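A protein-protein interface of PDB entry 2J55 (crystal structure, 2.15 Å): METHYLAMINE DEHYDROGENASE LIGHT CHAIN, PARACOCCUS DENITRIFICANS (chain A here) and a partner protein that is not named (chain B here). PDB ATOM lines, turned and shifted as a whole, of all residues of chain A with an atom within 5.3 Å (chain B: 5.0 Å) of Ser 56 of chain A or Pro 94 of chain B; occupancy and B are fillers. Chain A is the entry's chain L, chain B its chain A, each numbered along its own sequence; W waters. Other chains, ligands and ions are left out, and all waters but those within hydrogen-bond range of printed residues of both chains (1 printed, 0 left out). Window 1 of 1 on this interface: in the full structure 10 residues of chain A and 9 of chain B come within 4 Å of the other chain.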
ATOM      1  N   THR A  54       7.098  20.391  30.520  1.00  0.00           N
ATOM      2  CA  THR A  54       6.614  21.735  30.381  1.00  0.00           C
ATOM      3  C   THR A  54       6.729  22.126  28.909  1.00  0.00           C
ATOM      4  O   THR A  54       5.784  22.685  28.348  1.00  0.00           O
ATOM      5  CB  THR A  54       7.332  22.782  31.315  1.00  0.00           C
ATOM      6  OG1 THR A  54       8.685  22.950  30.876  1.00  0.00           O
ATOM      7  CG2 THR A  54       7.283  22.358  32.784  1.00  0.00           C
ATOM      8  N   ALA A  55       7.882  21.823  28.291  1.00  0.00           N
ATOM      9  CA  ALA A  55       8.145  22.273  26.912  1.00  0.00           C
ATOM     10  C   ALA A  55       7.419  21.402  25.934  1.00  0.00           C
ATOM     11  O   ALA A  55       6.855  20.332  26.306  1.00  0.00           O
ATOM     12  CB  ALA A  55       9.632  22.344  26.571  1.00  0.00           C
ATOM     13  N   SER A  56       7.405  21.868  24.697  1.00  0.00           N
ATOM     14  CA  SER A  56       6.787  21.101  23.669  1.00  0.00           C
ATOM     15  C   SER A  56       6.904  21.673  22.275  1.00  0.00           C
ATOM     16  O   SER A  56       7.425  22.778  22.077  1.00  0.00           O
ATOM     17  CB  SER A  56       5.340  20.742  24.045  1.00  0.00           C
ATOM     18  OG  SER A  56       4.391  21.603  23.492  1.00  0.00           O
ATOM     19  N   TRQ A  57       6.468  20.864  21.313  1.00  0.00           N
ATOM     20  CA  TRQ A  57       6.278  21.327  19.940  1.00  0.00           C
ATOM     21  C   TRQ A  57       4.824  21.757  19.892  1.00  0.00           C
ATOM     22  O   TRQ A  57       3.975  21.328  20.710  1.00  0.00           O
ATOM     23  CB  TRQ A  57       6.762  20.329  18.821  1.00  0.00           C
ATOM     24  CG  TRQ A  57       5.897  19.096  18.822  1.00  0.00           C
ATOM     25  CD1 TRQ A  57       4.726  18.968  18.081  1.00  0.00           C
ATOM     26  NE1 TRQ A  57       4.053  17.808  18.315  1.00  0.00           N
ATOM     27  CE2 TRQ A  57       4.774  17.053  19.183  1.00  0.00           C
ATOM     28  CZ2 TRQ A  57       4.564  15.727  19.803  1.00  0.00           C
ATOM     29  CH2 TRQ A  57       5.559  15.227  20.777  1.00  0.00           C
ATOM     30  CZ3 TRQ A  57       6.641  15.992  21.100  1.00  0.00           C
ATOM     31  CE3 TRQ A  57       6.854  17.253  20.529  1.00  0.00           C
ATOM     32  CD2 TRQ A  57       5.964  17.809  19.574  1.00  0.00           C
ATOM     33  O6  TRQ A  57       5.375  14.118  21.310  1.00  0.00           O
ATOM     34  O7  TRQ A  57       3.592  15.013  19.508  1.00  0.00           O
ATOM     35  N   VAL A  58       4.530  22.604  18.906  1.00  0.00           N
ATOM     36  CA  VAL A  58       3.160  23.135  18.673  1.00  0.00           C
ATOM     37  C   VAL A  58       2.780  22.984  17.228  1.00  0.00           C
ATOM     38  O   VAL A  58       3.632  22.918  16.375  1.00  0.00           O
ATOM     39  CB  VAL A  58       2.978  24.660  19.142  1.00  0.00           C
ATOM     40  CG1 VAL A  58       3.279  24.758  20.619  1.00  0.00           C
ATOM     41  CG2 VAL A  58       3.905  25.607  18.417  1.00  0.00           C
ATOM     42  N   ALA A  73      -0.320  22.505  22.282  1.00  0.00           N
ATOM     43  CA  ALA A  73       1.013  22.228  22.855  1.00  0.00           C
ATOM     44  C   ALA A  73       1.066  20.750  23.181  1.00  0.00           C
ATOM     45  O   ALA A  73       0.388  20.256  24.107  1.00  0.00           O
ATOM     46  CB  ALA A  73       1.301  23.034  24.071  1.00  0.00           C
ATOM     47  N   TYR A  74       1.850  20.043  22.375  1.00  0.00           N
ATOM     48  CA  TYR A  74       2.016  18.640  22.534  1.00  0.00           C
ATOM     49  C   TYR A  74       3.125  18.378  23.545  1.00  0.00           C
ATOM     50  O   TYR A  74       4.277  18.095  23.184  1.00  0.00           O
ATOM     51  CB  TYR A  74       2.340  17.992  21.182  1.00  0.00           C
ATOM     52  CG  TYR A  74       1.229  18.165  20.171  1.00  0.00           C
ATOM     53  CD1 TYR A  74       0.097  17.344  20.210  1.00  0.00           C
ATOM     54  CD2 TYR A  74       1.316  19.143  19.170  1.00  0.00           C
ATOM     55  CE1 TYR A  74      -0.897  17.483  19.296  1.00  0.00           C
ATOM     56  CE2 TYR A  74       0.307  19.307  18.258  1.00  0.00           C
ATOM     57  CZ  TYR A  74      -0.784  18.476  18.333  1.00  0.00           C
ATOM     58  OH  TYR A  74      -1.779  18.615  17.423  1.00  0.00           O
ATOM     59  N   ARG A  75       2.756  18.459  24.820  1.00  0.00           N
ATOM     60  CA  ARG A  75       3.640  18.108  25.923  1.00  0.00           C
ATOM     61  C   ARG A  75       3.495  16.617  26.173  1.00  0.00           C
ATOM     62  O   ARG A  75       2.378  16.030  26.070  1.00  0.00           O
ATOM     63  CB  ARG A  75       3.279  18.886  27.194  1.00  0.00           C
ATOM     64  CG  ARG A  75       3.237  20.366  26.974  1.00  0.00           C
ATOM     65  CD  ARG A  75       2.282  21.079  27.978  1.00  0.00           C
ATOM     66  NE  ARG A  75       2.799  20.960  29.343  1.00  0.00           N
ATOM     67  CZ  ARG A  75       2.248  21.497  30.437  1.00  0.00           C
ATOM     68  NH1 ARG A  75       1.111  22.182  30.345  1.00  0.00           N
ATOM     69  NH2 ARG A  75       2.832  21.329  31.616  1.00  0.00           N
ATOM     70  N   PRO A 100      12.631  23.604  15.464  1.00  0.00           N
ATOM     71  CA  PRO A 100      12.184  22.695  16.512  1.00  0.00           C
ATOM     72  C   PRO A 100      10.811  22.990  17.065  1.00  0.00           C
ATOM     73  O   PRO A 100      10.147  22.053  17.552  1.00  0.00           O
ATOM     74  CB  PRO A 100      13.294  22.722  17.584  1.00  0.00           C
ATOM     75  CG  PRO A 100      14.263  23.814  17.159  1.00  0.00           C
ATOM     76  CD  PRO A 100      13.933  24.227  15.715  1.00  0.00           C
ATOM     77  N   GLU A 101      10.360  24.261  16.968  1.00  0.00           N
ATOM     78  CA  GLU A 101       9.108  24.720  17.610  1.00  0.00           C
ATOM     79  C   GLU A 101       7.891  23.981  17.107  1.00  0.00           C
ATOM     80  O   GLU A 101       6.880  23.776  17.827  1.00  0.00           O
ATOM     81  CB  GLU A 101       8.899  26.264  17.433  1.00  0.00           C
ATOM     82  CG  GLU A 101       8.968  26.882  15.985  1.00  0.00           C
ATOM     83  CD  GLU A 101      10.376  27.077  15.530  1.00  0.00           C
ATOM     84  OE1 GLU A 101      11.285  26.412  16.077  1.00  0.00           O
ATOM     85  OE2 GLU A 101      10.598  27.889  14.628  1.00  0.00           O
ATOM     86  N   TRP A 108       9.473  15.436  23.689  1.00  0.00           N
ATOM     87  CA  TRP A 108       9.175  16.761  24.266  1.00  0.00           C
ATOM     88  C   TRP A 108       8.970  16.626  25.769  1.00  0.00           C
ATOM     89  O   TRP A 108       7.847  16.671  26.263  1.00  0.00           O
ATOM     90  CB  TRP A 108       8.064  17.541  23.498  1.00  0.00           C
ATOM     91  CG  TRP A 108       8.608  18.256  22.198  1.00  0.00           C
ATOM     92  CD1 TRP A 108       8.193  18.075  20.847  1.00  0.00           C
ATOM     93  CD2 TRP A 108       9.659  19.183  22.145  1.00  0.00           C
ATOM     94  NE1 TRP A 108       8.943  18.858  20.009  1.00  0.00           N
ATOM     95  CE2 TRP A 108       9.835  19.562  20.770  1.00  0.00           C
ATOM     96  CE3 TRP A 108      10.460  19.777  23.121  1.00  0.00           C
ATOM     97  CZ2 TRP A 108      10.828  20.477  20.369  1.00  0.00           C
ATOM     98  CZ3 TRP A 108      11.409  20.695  22.720  1.00  0.00           C
ATOM     99  CH2 TRP A 108      11.599  21.035  21.352  1.00  0.00           C
ATOM    100  N   PRO B  52       4.188  29.214  23.190  1.00  0.00           N
ATOM    101  CA  PRO B  52       4.783  29.267  24.568  1.00  0.00           C
ATOM    102  C   PRO B  52       6.285  29.459  24.549  1.00  0.00           C
ATOM    103  O   PRO B  52       6.904  28.983  23.628  1.00  0.00           O
ATOM    104  CB  PRO B  52       4.348  27.956  25.207  1.00  0.00           C
ATOM    105  CG  PRO B  52       3.011  27.678  24.484  1.00  0.00           C
ATOM    106  CD  PRO B  52       3.340  28.028  23.010  1.00  0.00           C
ATOM    107  N   ASN B  54       9.770  30.446  27.677  1.00  0.00           N
ATOM    108  CA  ASN B  54      10.090  30.682  29.076  1.00  0.00           C
ATOM    109  C   ASN B  54      11.498  31.223  29.102  1.00  0.00           C
ATOM    110  O   ASN B  54      12.072  31.431  28.033  1.00  0.00           O
ATOM    111  CB  ASN B  54       9.930  29.361  29.917  1.00  0.00           C
ATOM    112  CG  ASN B  54      11.023  28.349  29.641  1.00  0.00           C
ATOM    113  OD1 ASN B  54      11.745  28.457  28.656  1.00  0.00           O
ATOM    114  ND2 ASN B  54      11.172  27.367  30.539  1.00  0.00           N
ATOM    115  N   MET B  71       6.376  28.039  31.331  1.00  0.00           N
ATOM    116  CA  MET B  71       5.953  28.514  30.026  1.00  0.00           C
ATOM    117  C   MET B  71       4.863  29.536  30.203  1.00  0.00           C
ATOM    118  O   MET B  71       3.840  29.330  30.909  1.00  0.00           O
ATOM    119  CB  MET B  71       5.416  27.395  29.082  1.00  0.00           C
ATOM    120  CG  MET B  71       6.360  26.183  28.833  1.00  0.00           C
ATOM    121  SD  MET B  71       8.122  26.481  28.388  1.00  0.00           S
ATOM    122  CE  MET B  71       8.024  27.195  26.762  1.00  0.00           C
ATOM    123  N   CYS B  92      15.383  29.746  26.109  1.00  0.00           N
ATOM    124  CA  CYS B  92      14.034  29.210  26.226  1.00  0.00           C
ATOM    125  C   CYS B  92      14.115  27.667  26.112  1.00  0.00           C
ATOM    126  O   CYS B  92      14.853  27.129  25.259  1.00  0.00           O
ATOM    127  CB  CYS B  92      13.217  29.760  25.072  1.00  0.00           C
ATOM    128  SG  CYS B  92      11.518  29.161  25.011  1.00  0.00           S
ATOM    129  N   THR B  93      13.316  26.972  26.921  1.00  0.00           N
ATOM    130  CA  THR B  93      13.518  25.536  27.119  1.00  0.00           C
ATOM    131  C   THR B  93      13.260  24.751  25.797  1.00  0.00           C
ATOM    132  O   THR B  93      14.214  24.128  25.315  1.00  0.00           O
ATOM    133  CB  THR B  93      12.776  24.983  28.389  1.00  0.00           C
ATOM    134  OG1 THR B  93      13.397  25.537  29.558  1.00  0.00           O
ATOM    135  CG2 THR B  93      12.869  23.437  28.443  1.00  0.00           C
ATOM    136  N   PRO B  94      12.022  24.859  25.179  1.00  0.00           N
ATOM    137  CA  PRO B  94      11.815  24.219  23.845  1.00  0.00           C
ATOM    138  C   PRO B  94      12.615  24.844  22.705  1.00  0.00           C
ATOM    139  O   PRO B  94      12.813  24.194  21.695  1.00  0.00           O
ATOM    140  CB  PRO B  94      10.294  24.359  23.592  1.00  0.00           C
ATOM    141  CG  PRO B  94       9.855  25.581  24.405  1.00  0.00           C
ATOM    142  CD  PRO B  94      10.762  25.466  25.673  1.00  0.00           C
ATOM    143  N   HIS B  95      13.085  26.087  22.877  1.00  0.00           N
ATOM    144  CA  HIS B  95      13.694  26.846  21.750  1.00  0.00           C
ATOM    145  C   HIS B  95      15.106  27.384  21.992  1.00  0.00           C
ATOM    146  O   HIS B  95      15.290  28.611  22.133  1.00  0.00           O
ATOM    147  CB  HIS B  95      12.740  27.952  21.309  1.00  0.00           C
ATOM    148  CG  HIS B  95      11.332  27.469  21.131  1.00  0.00           C
ATOM    149  ND1 HIS B  95      10.248  28.098  21.674  1.00  0.00           N
ATOM    150  CD2 HIS B  95      10.840  26.366  20.509  1.00  0.00           C
ATOM    151  CE1 HIS B  95       9.140  27.434  21.401  1.00  0.00           C
ATOM    152  NE2 HIS B  95       9.473  26.366  20.688  1.00  0.00           N
ATOM    153  N   PRO B  96      16.133  26.497  22.054  1.00  0.00           N
ATOM    154  CA  PRO B  96      17.501  26.917  22.579  1.00  0.00           C
ATOM    155  C   PRO B  96      18.267  27.876  21.670  1.00  0.00           C
ATOM    156  O   PRO B  96      19.357  28.378  22.024  1.00  0.00           O
ATOM    157  CB  PRO B  96      18.249  25.570  22.803  1.00  0.00           C
ATOM    158  CG  PRO B  96      17.521  24.618  21.912  1.00  0.00           C
ATOM    159  CD  PRO B  96      16.080  25.064  21.744  1.00  0.00           C
HETATM  160  O   HOH W   1       7.248  24.728  20.482  1.00  0.00           O
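Among the printed residues, pairs that only touch across the chains: Thr 54 of chain A with Met 71 of chain B, Ala 55 of chain A with Thr 93 of chain B, Ala 55 of chain A with Pro 94 of chain B, Ser 56 of chain A with Pro 94 of chain B, Glu 101 of chain A with His 95 of chain B and Trp 108 of chain A with Pro 94 of chain B.
Water W1 lies within hydrogen-bond range of O of Ser 56 of chain A (2.5 Å), NE2 of His 95 of chain B (2.8 Å) and O of Glu 101 of chain A (2.8 Å).
Of the 11 printed residues of chain A, 5 touch a printed residue of chain B.
Printed residues of chain B that touch a printed residue of chain A: Met 71, Thr 93, Pro 94 and His 95.
Among the printed residues, 6 pairs touch across the chains.
Of chain B, only Pro 94 comes within 4 Å of Ser 56 of chain A.
Pro 94 of chain B touches just these residues of chain A: Ala 55, Ser 56 and Trp 108.
Printed residues of chain B within 4 Å of Trp 108 of chain A: Pro 94 (3.4 Å).
Of the printed residues of chain A, Thr 93 of chain B touches Ala 55 (3.9 Å).
Of the printed residues of chain B, Thr 54 of chain A touches Met 71 (3.6 Å).
Tyr 74 of chain A touches none of the printed residues of chain B.
The nearest residue of chain B that does not touch Ser 56 of chain A is His 95 of chain B (4.4 Å).
The nearest residue of chain A that does not touch Pro 94 of chain B is Pro 100 of chain A (4.4 Å).
N of Val 58 of chain A is in hydrogen-bond range of O of Glu 101 of chain A (2.8 Å).
N of Thr 93 of chain B is in hydrogen-bond range of OD1 of Asn 54 of chain B (2.8 Å).
CD1 of Trp 108 of chain A is covalently linked to CE3 of TRQ 57 of chain A (1.6 Å).
The side-chain hydroxyl of Ser 56 of chain A lies within hydrogen-bond range of the backbone NH of Tyr 74 of chain A (3.2 Å).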
